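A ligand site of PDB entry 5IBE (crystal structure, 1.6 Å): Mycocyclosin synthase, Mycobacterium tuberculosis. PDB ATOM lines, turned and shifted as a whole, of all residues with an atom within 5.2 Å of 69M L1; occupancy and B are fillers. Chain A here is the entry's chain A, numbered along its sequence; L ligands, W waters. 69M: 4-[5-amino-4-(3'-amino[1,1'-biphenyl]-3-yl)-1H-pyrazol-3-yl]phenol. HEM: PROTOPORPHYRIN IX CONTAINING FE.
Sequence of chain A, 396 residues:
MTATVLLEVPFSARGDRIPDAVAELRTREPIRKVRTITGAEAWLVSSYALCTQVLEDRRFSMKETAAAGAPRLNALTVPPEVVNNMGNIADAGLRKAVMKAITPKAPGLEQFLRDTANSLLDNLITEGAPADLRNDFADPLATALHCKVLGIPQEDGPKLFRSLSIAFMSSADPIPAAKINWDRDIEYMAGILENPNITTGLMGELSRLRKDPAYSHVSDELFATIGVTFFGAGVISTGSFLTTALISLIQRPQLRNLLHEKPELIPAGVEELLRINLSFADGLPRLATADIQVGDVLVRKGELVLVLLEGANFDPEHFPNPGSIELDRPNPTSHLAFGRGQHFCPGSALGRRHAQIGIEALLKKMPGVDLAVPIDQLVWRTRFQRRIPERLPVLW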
ATOM      1  N   MET A  62      26.013  33.938 -31.265  1.00  0.00           N
ATOM      2  CA  MET A  62      24.844  33.061 -31.151  1.00  0.00           C
ATOM      3  C   MET A  62      23.612  33.919 -30.913  1.00  0.00           C
ATOM      4  O   MET A  62      22.595  33.765 -31.586  1.00  0.00           O
ATOM      5  CB  MET A  62      24.996  32.043 -30.004  1.00  0.00           C
ATOM      6  CG  MET A  62      23.684  31.316 -29.654  1.00  0.00           C
ATOM      7  SD  MET A  62      23.812  30.207 -28.238  1.00  0.00           S
ATOM      8  CE  MET A  62      24.949  28.992 -28.884  1.00  0.00           C
ATOM      9  N   LEU A  76      12.679  30.057 -35.253  1.00  0.00           N
ATOM     10  CA  LEU A  76      12.697  29.933 -33.804  1.00  0.00           C
ATOM     11  C   LEU A  76      11.562  29.033 -33.322  1.00  0.00           C
ATOM     12  O   LEU A  76      10.426  29.140 -33.772  1.00  0.00           O
ATOM     13  CB  LEU A  76      12.561  31.311 -33.157  1.00  0.00           C
ATOM     14  CG  LEU A  76      13.789  32.216 -33.280  1.00  0.00           C
ATOM     15  CD1 LEU A  76      13.414  33.619 -32.846  1.00  0.00           C
ATOM     16  CD2 LEU A  76      14.941  31.687 -32.460  1.00  0.00           C
ATOM     17  N   THR A  77      11.891  28.150 -32.376  1.00  0.00           N
ATOM     18  CA  THR A  77      10.884  27.331 -31.715  1.00  0.00           C
ATOM     19  C   THR A  77      10.736  27.746 -30.253  1.00  0.00           C
ATOM     20  O   THR A  77      10.058  27.072 -29.474  1.00  0.00           O
ATOM     21  CB  THR A  77      11.231  25.841 -31.790  1.00  0.00           C
ATOM     22  OG1 THR A  77      12.465  25.609 -31.103  1.00  0.00           O
ATOM     23  CG2 THR A  77      11.383  25.401 -33.236  1.00  0.00           C
ATOM     24  N   VAL A  78      11.376  28.857 -29.902  1.00  0.00           N
ATOM     25  CA  VAL A  78      11.342  29.406 -28.549  1.00  0.00           C
ATOM     26  C   VAL A  78      11.260  30.922 -28.639  1.00  0.00           C
ATOM     27  O   VAL A  78      11.526  31.491 -29.691  1.00  0.00           O
ATOM     28  CB  VAL A  78      12.595  29.033 -27.736  1.00  0.00           C
ATOM     29  CG1 VAL A  78      12.610  27.541 -27.456  1.00  0.00           C
ATOM     30  CG2 VAL A  78      13.869  29.447 -28.484  1.00  0.00           C
ATOM     31  N   VAL A  82      15.374  33.038 -25.288  1.00  0.00           N
ATOM     32  CA  VAL A  82      15.845  31.705 -24.913  1.00  0.00           C
ATOM     33  C   VAL A  82      17.114  31.339 -25.677  1.00  0.00           C
ATOM     34  O   VAL A  82      17.906  30.512 -25.239  1.00  0.00           O
ATOM     35  CB  VAL A  82      14.743  30.658 -25.162  1.00  0.00           C
ATOM     36  CG1 VAL A  82      15.242  29.243 -24.890  1.00  0.00           C
ATOM     37  CG2 VAL A  82      13.532  30.965 -24.292  1.00  0.00           C
ATOM     38  N   VAL A  83      17.320  31.977 -26.832  1.00  0.00           N
ATOM     39  CA  VAL A  83      18.508  31.718 -27.625  1.00  0.00           C
ATOM     40  C   VAL A  83      19.755  32.100 -26.821  1.00  0.00           C
ATOM     41  O   VAL A  83      20.792  31.448 -26.920  1.00  0.00           O
ATOM     42  CB  VAL A  83      18.474  32.484 -28.954  1.00  0.00           C
ATOM     43  CG1 VAL A  83      19.820  32.427 -29.683  1.00  0.00           C
ATOM     44  CG2 VAL A  83      17.368  31.908 -29.843  1.00  0.00           C
ATOM     45  N   ASN A  85      20.018  31.893 -23.547  1.00  0.00           N
ATOM     46  CA  ASN A  85      19.695  31.394 -22.214  1.00  0.00           C
ATOM     47  C   ASN A  85      20.916  31.354 -21.297  1.00  0.00           C
ATOM     48  O   ASN A  85      20.851  31.833 -20.175  1.00  0.00           O
ATOM     49  CB  ASN A  85      19.059  30.003 -22.288  1.00  0.00           C
ATOM     50  CG  ASN A  85      18.509  29.525 -20.941  1.00  0.00           C
ATOM     51  OD1 ASN A  85      18.879  28.473 -20.439  1.00  0.00           O
ATOM     52  ND2 ASN A  85      17.632  30.336 -20.353  1.00  0.00           N
ATOM     53  N   ALA A 167       9.719  20.474 -30.457  1.00  0.00           N
ATOM     54  CA  ALA A 167      10.560  21.544 -29.921  1.00  0.00           C
ATOM     55  C   ALA A 167      11.891  21.675 -30.655  1.00  0.00           C
ATOM     56  O   ALA A 167      12.415  22.778 -30.835  1.00  0.00           O
ATOM     57  CB  ALA A 167      10.804  21.323 -28.442  1.00  0.00           C
ATOM     58  N   PHE A 168      12.445  20.548 -31.096  1.00  0.00           N
ATOM     59  CA  PHE A 168      13.752  20.567 -31.741  1.00  0.00           C
ATOM     60  C   PHE A 168      13.660  20.292 -33.238  1.00  0.00           C
ATOM     61  O   PHE A 168      14.613  19.853 -33.862  1.00  0.00           O
ATOM     62  CB  PHE A 168      14.681  19.591 -31.013  1.00  0.00           C
ATOM     63  CG  PHE A 168      15.153  20.145 -29.700  1.00  0.00           C
ATOM     64  CD1 PHE A 168      14.431  19.911 -28.546  1.00  0.00           C
ATOM     65  CD2 PHE A 168      16.260  20.969 -29.647  1.00  0.00           C
ATOM     66  CE1 PHE A 168      14.839  20.451 -27.341  1.00  0.00           C
ATOM     67  CE2 PHE A 168      16.667  21.518 -28.439  1.00  0.00           C
ATOM     68  CZ  PHE A 168      15.961  21.255 -27.290  1.00  0.00           C
ATOM     69  N   TRP A 182       5.549  24.812 -25.384  1.00  0.00           N
ATOM     70  CA  TRP A 182       6.472  25.658 -24.636  1.00  0.00           C
ATOM     71  C   TRP A 182       5.746  26.328 -23.467  1.00  0.00           C
ATOM     72  O   TRP A 182       6.207  26.273 -22.322  1.00  0.00           O
ATOM     73  CB  TRP A 182       7.108  26.711 -25.541  1.00  0.00           C
ATOM     74  CG  TRP A 182       8.000  27.647 -24.787  1.00  0.00           C
ATOM     75  CD1 TRP A 182       7.674  28.882 -24.304  1.00  0.00           C
ATOM     76  CD2 TRP A 182       9.351  27.415 -24.393  1.00  0.00           C
ATOM     77  NE1 TRP A 182       8.743  29.434 -23.657  1.00  0.00           N
ATOM     78  CE2 TRP A 182       9.791  28.556 -23.696  1.00  0.00           C
ATOM     79  CE3 TRP A 182      10.248  26.349 -24.573  1.00  0.00           C
ATOM     80  CZ2 TRP A 182      11.077  28.658 -23.175  1.00  0.00           C
ATOM     81  CZ3 TRP A 182      11.520  26.461 -24.051  1.00  0.00           C
ATOM     82  CH2 TRP A 182      11.923  27.609 -23.352  1.00  0.00           C
ATOM     83  N   THR A 229      14.473  24.577 -20.804  1.00  0.00           N
ATOM     84  CA  THR A 229      15.581  24.568 -21.754  1.00  0.00           C
ATOM     85  C   THR A 229      16.587  23.467 -21.434  1.00  0.00           C
ATOM     86  O   THR A 229      17.050  22.750 -22.331  1.00  0.00           O
ATOM     87  CB  THR A 229      16.314  25.929 -21.767  1.00  0.00           C
ATOM     88  OG1 THR A 229      15.383  26.965 -22.130  1.00  0.00           O
ATOM     89  CG2 THR A 229      17.467  25.935 -22.756  1.00  0.00           C
ATOM     90  N   ALA A 233      17.051  20.373 -23.977  1.00  0.00           N
ATOM     91  CA  ALA A 233      18.332  20.289 -24.667  1.00  0.00           C
ATOM     92  C   ALA A 233      19.137  19.090 -24.168  1.00  0.00           C
ATOM     93  O   ALA A 233      19.764  18.383 -24.955  1.00  0.00           O
ATOM     94  CB  ALA A 233      19.124  21.560 -24.470  1.00  0.00           C
ATOM     95  N   GLY A 234      19.099  18.860 -22.868  1.00  0.00           N
ATOM     96  CA  GLY A 234      19.836  17.757 -22.286  1.00  0.00           C
ATOM     97  C   GLY A 234      19.329  16.407 -22.751  1.00  0.00           C
ATOM     98  O   GLY A 234      20.102  15.552 -23.178  1.00  0.00           O
ATOM     99  N   SER A 237      19.782  15.840 -26.566  1.00  0.00           N
ATOM    100  CA  SER A 237      21.185  15.700 -26.932  1.00  0.00           C
ATOM    101  C   SER A 237      21.747  14.350 -26.476  1.00  0.00           C
ATOM    102  O   SER A 237      22.401  13.663 -27.251  1.00  0.00           O
ATOM    103  CB  SER A 237      22.009  16.850 -26.352  1.00  0.00           C
ATOM    104  OG  SER A 237      21.588  18.099 -26.893  1.00  0.00           O
ATOM    105  N   PHE A 280      24.144  15.989 -34.720  1.00  0.00           N
ATOM    106  CA  PHE A 280      23.720  17.338 -35.074  1.00  0.00           C
ATOM    107  C   PHE A 280      23.408  17.422 -36.564  1.00  0.00           C
ATOM    108  O   PHE A 280      24.288  17.199 -37.407  1.00  0.00           O
ATOM    109  CB  PHE A 280      24.765  18.383 -34.686  1.00  0.00           C
ATOM    110  CG  PHE A 280      24.644  18.841 -33.257  1.00  0.00           C
ATOM    111  CD1 PHE A 280      24.924  17.976 -32.210  1.00  0.00           C
ATOM    112  CD2 PHE A 280      24.199  20.114 -32.967  1.00  0.00           C
ATOM    113  CE1 PHE A 280      24.799  18.396 -30.900  1.00  0.00           C
ATOM    114  CE2 PHE A 280      24.073  20.544 -31.654  1.00  0.00           C
ATOM    115  CZ  PHE A 280      24.364  19.676 -30.629  1.00  0.00           C
ATOM    116  N   CYS A 345      29.376  23.315 -24.405  1.00  0.00           N
ATOM    117  CA  CYS A 345      28.307  22.633 -23.691  1.00  0.00           C
ATOM    118  C   CYS A 345      28.574  22.521 -22.188  1.00  0.00           C
ATOM    119  O   CYS A 345      29.586  21.939 -21.782  1.00  0.00           O
ATOM    120  CB  CYS A 345      28.094  21.237 -24.249  1.00  0.00           C
ATOM    121  SG  CYS A 345      26.720  20.371 -23.479  1.00  0.00           S
ATOM    122  N   GLN A 385      16.572  19.002 -35.549  1.00  0.00           N
ATOM    123  CA  GLN A 385      17.879  19.529 -35.186  1.00  0.00           C
ATOM    124  C   GLN A 385      18.860  18.421 -34.850  1.00  0.00           C
ATOM    125  O   GLN A 385      20.054  18.668 -34.701  1.00  0.00           O
ATOM    126  CB  GLN A 385      17.763  20.503 -34.019  1.00  0.00           C
ATOM    127  CG  GLN A 385      17.035  21.788 -34.400  1.00  0.00           C
ATOM    128  CD  GLN A 385      16.849  22.729 -33.242  1.00  0.00           C
ATOM    129  OE1 GLN A 385      17.712  22.868 -32.379  1.00  0.00           O
ATOM    130  NE2 GLN A 385      15.691  23.394 -33.216  1.00  0.00           N
ATOM    131  N   ARG A 386      18.347  17.198 -34.720  1.00  0.00           N
ATOM    132  CA  ARG A 386      19.193  16.020 -34.569  1.00  0.00           C
ATOM    133  C   ARG A 386      18.918  15.007 -35.660  1.00  0.00           C
ATOM    134  O   ARG A 386      17.823  14.975 -36.235  1.00  0.00           O
ATOM    135  CB  ARG A 386      18.988  15.364 -33.208  1.00  0.00           C
ATOM    136  CG  ARG A 386      19.359  16.217 -32.011  1.00  0.00           C
ATOM    137  CD  ARG A 386      20.845  16.512 -31.955  1.00  0.00           C
ATOM    138  NE  ARG A 386      21.153  17.310 -30.765  1.00  0.00           N
ATOM    139  CZ  ARG A 386      20.990  18.628 -30.700  1.00  0.00           C
ATOM    140  NH1 ARG A 386      20.548  19.305 -31.754  1.00  0.00           N
ATOM    141  NH2 ARG A 386      21.277  19.279 -29.582  1.00  0.00           N
HETATM  142  C2  69M L   1      14.911  25.008 -26.302  1.00  0.00           C
HETATM  143  C4  69M L   1      15.967  25.949 -28.249  1.00  0.00           C
HETATM  144  C5  69M L   1      15.071  25.260 -29.063  1.00  0.00           C
HETATM  145  C6  69M L   1      14.098  24.451 -28.498  1.00  0.00           C
HETATM  146  C8  69M L   1      18.383  27.122 -28.474  1.00  0.00           C
HETATM  147  C9  69M L   1      18.814  28.052 -29.540  1.00  0.00           C
HETATM  148  C12 69M L   1      19.206  26.596 -27.350  1.00  0.00           C
HETATM  149  C13 69M L   1      19.204  27.151 -26.079  1.00  0.00           C
HETATM  150  C14 69M L   1      20.011  26.590 -25.089  1.00  0.00           C
HETATM  151  C15 69M L   1      20.823  25.489 -25.380  1.00  0.00           C
HETATM  152  C1  69M L   1      14.014  24.329 -27.113  1.00  0.00           C
HETATM  153  C3  69M L   1      15.891  25.829 -26.870  1.00  0.00           C
HETATM  154  O1  69M L   1      13.050  23.545 -26.561  1.00  0.00           O
HETATM  155  C7  69M L   1      16.993  26.817 -28.899  1.00  0.00           C
HETATM  156  N10 69M L   1      17.858  28.320 -30.424  1.00  0.00           N
HETATM  157  N11 69M L   1      16.736  27.558 -30.017  1.00  0.00           N
HETATM  158  C16 69M L   1      20.808  24.959 -26.670  1.00  0.00           C
HETATM  159  C17 69M L   1      20.012  25.516 -27.644  1.00  0.00           C
HETATM  160  C18 69M L   1      21.626  23.793 -27.093  1.00  0.00           C
HETATM  161  C19 69M L   1      21.877  22.725 -26.250  1.00  0.00           C
HETATM  162  C20 69M L   1      22.633  21.655 -26.694  1.00  0.00           C
HETATM  163  C21 69M L   1      23.115  21.636 -28.005  1.00  0.00           C
HETATM  164  C22 69M L   1      22.851  22.694 -28.853  1.00  0.00           C
HETATM  165  C23 69M L   1      22.108  23.774 -28.404  1.00  0.00           C
HETATM  166  N24 69M L   1      20.143  28.635 -29.577  1.00  0.00           N
HETATM  167  N25 69M L   1      22.907  20.507 -25.788  1.00  0.00           N
HETATM  168  CHA HEM L   2      25.569  23.691 -25.825  1.00  0.00           C
HETATM  169  CHB HEM L   2      26.237  19.255 -27.635  1.00  0.00           C
HETATM  170  CHC HEM L   2      24.489  17.406 -23.515  1.00  0.00           C
HETATM  171  CHD HEM L   2      22.838  21.750 -22.261  1.00  0.00           C
HETATM  172  C1A HEM L   2      25.954  22.664 -26.646  1.00  0.00           C
HETATM  173  C2A HEM L   2      26.681  22.799 -27.890  1.00  0.00           C
HETATM  174  C3A HEM L   2      26.858  21.580 -28.390  1.00  0.00           C
HETATM  175  C4A HEM L   2      26.264  20.622 -27.478  1.00  0.00           C
HETATM  176  CMA HEM L   2      27.577  21.226 -29.712  1.00  0.00           C
HETATM  177  CAA HEM L   2      27.156  24.134 -28.513  1.00  0.00           C
HETATM  178  CBA HEM L   2      26.010  24.842 -29.231  1.00  0.00           C
HETATM  179  CGA HEM L   2      26.544  26.056 -29.963  1.00  0.00           C
HETATM  180  O1A HEM L   2      27.695  26.470 -29.680  1.00  0.00           O
HETATM  181  O2A HEM L   2      25.806  26.596 -30.832  1.00  0.00           O
HETATM  182  C1B HEM L   2      25.846  18.366 -26.662  1.00  0.00           C
HETATM  183  C2B HEM L   2      25.994  16.931 -26.721  1.00  0.00           C
HETATM  184  C3B HEM L   2      25.493  16.413 -25.580  1.00  0.00           C
HETATM  185  C4B HEM L   2      25.036  17.520 -24.764  1.00  0.00           C
HETATM  186  CMB HEM L   2      26.588  16.206 -27.949  1.00  0.00           C
HETATM  187  CAB HEM L   2      25.379  14.945 -25.092  1.00  0.00           C
HETATM  188  CBB HEM L   2      26.047  13.919 -25.637  1.00  0.00           C
HETATM  189  C1C HEM L   2      23.908  18.419 -22.798  1.00  0.00           C
HETATM  190  C2C HEM L   2      23.273  18.286 -21.504  1.00  0.00           C
HETATM  191  C3C HEM L   2      22.814  19.496 -21.146  1.00  0.00           C
HETATM  192  C4C HEM L   2      23.146  20.411 -22.221  1.00  0.00           C
HETATM  193  CMC HEM L   2      23.218  16.929 -20.744  1.00  0.00           C
HETATM  194  CAC HEM L   2      22.056  19.992 -19.886  1.00  0.00           C
HETATM  195  CBC HEM L   2      21.559  19.194 -18.928  1.00  0.00           C
HETATM  196  C1D HEM L   2      23.422  22.681 -23.085  1.00  0.00           C
HETATM  197  C2D HEM L   2      23.219  24.106 -23.001  1.00  0.00           C
HETATM  198  C3D HEM L   2      24.072  24.710 -24.106  1.00  0.00           C
HETATM  199  C4D HEM L   2      24.706  23.589 -24.763  1.00  0.00           C
HETATM  200  CMD HEM L   2      22.336  24.863 -21.987  1.00  0.00           C
HETATM  201  CAD HEM L   2      24.214  26.200 -24.446  1.00  0.00           C
HETATM  202  CBD HEM L   2      25.587  26.669 -23.982  1.00  0.00           C
HETATM  203  CGD HEM L   2      25.762  28.146 -24.199  1.00  0.00           C
HETATM  204  O1D HEM L   2      26.674  28.753 -23.565  1.00  0.00           O
HETATM  205  O2D HEM L   2      25.003  28.738 -25.004  1.00  0.00           O
HETATM  206  NA  HEM L   2      25.712  21.327 -26.421  1.00  0.00           N
HETATM  207  NB  HEM L   2      25.272  18.690 -25.448  1.00  0.00           N
HETATM  208  NC  HEM L   2      23.816  19.728 -23.218  1.00  0.00           N
HETATM  209  ND  HEM L   2      24.301  22.415 -24.137  1.00  0.00           N
HETATM  210 FE   HEM L   2      24.844  20.529 -24.770  1.00  0.00          FE
HETATM  211  O   HOH W   1      20.919  29.971 -32.400  1.00  0.00           O
HETATM  212  O   HOH W   2      10.419  24.628 -28.153  1.00  0.00           O
HETATM  213  O   HOH W   3      13.212  22.466 -24.390  1.00  0.00           O
HETATM  214  O   HOH W   4      14.519  27.360 -31.741  1.00  0.00           O
HETATM  215  O   HOH W   5      17.713  29.405 -32.717  1.00  0.00           O
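The side-chain hydroxyl of Ser 237 lies close to a nitrogen (N25) of 69M L1. An iron atom (FE) of HEM L2 is bound by the side-chain sulfur of Cys 345.
A nitrogen (N25) of 69M L1 binds an iron atom (FE) of HEM L2.
OG of Ser 237 lies within hydrogen-bond range of NH2 of Arg 386 (3.0 Å). The side-chain hydroxyl of Ser 237 lies within hydrogen-bond range of the backbone carbonyl oxygen of Ala 233 (2.7 Å). The side-chain hydroxyl (OG1) of Thr 77 lies within hydrogen-bond range of the backbone carbonyl oxygen (O) of Ala 167 (2.8 Å). N of Gln 385 is in hydrogen-bond range of O of Phe 168 (2.7 Å).
Merely in contact with 69M L1: Thr 77, Ala 167, Arg 386, Ala 233, Phe 280, Thr 229, Val 78, Phe 168, Val 83 and Val 82. Hydrophobic or aromatic side chains within 4 Å of 69M L1: Val 78, Val 82, Val 83, Ala 167, Phe 168, Ala 233 and Phe 280. Of the 18 residues printed, 11 come within 4 Å of 69M L1. The nearest printed residue that does not touch 69M L1 is Trp 182 (4.1 Å).
Water W4 lies within hydrogen-bond range of the side-chain hydroxyl (OG1) of Thr 77 (2.8 Å) and a nitrogen (N11) of 69M L1 (2.8 Å). Water W2 bridges O of Thr 77 (2.8 Å) and O1 of 69M L1 (3.3 Å).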
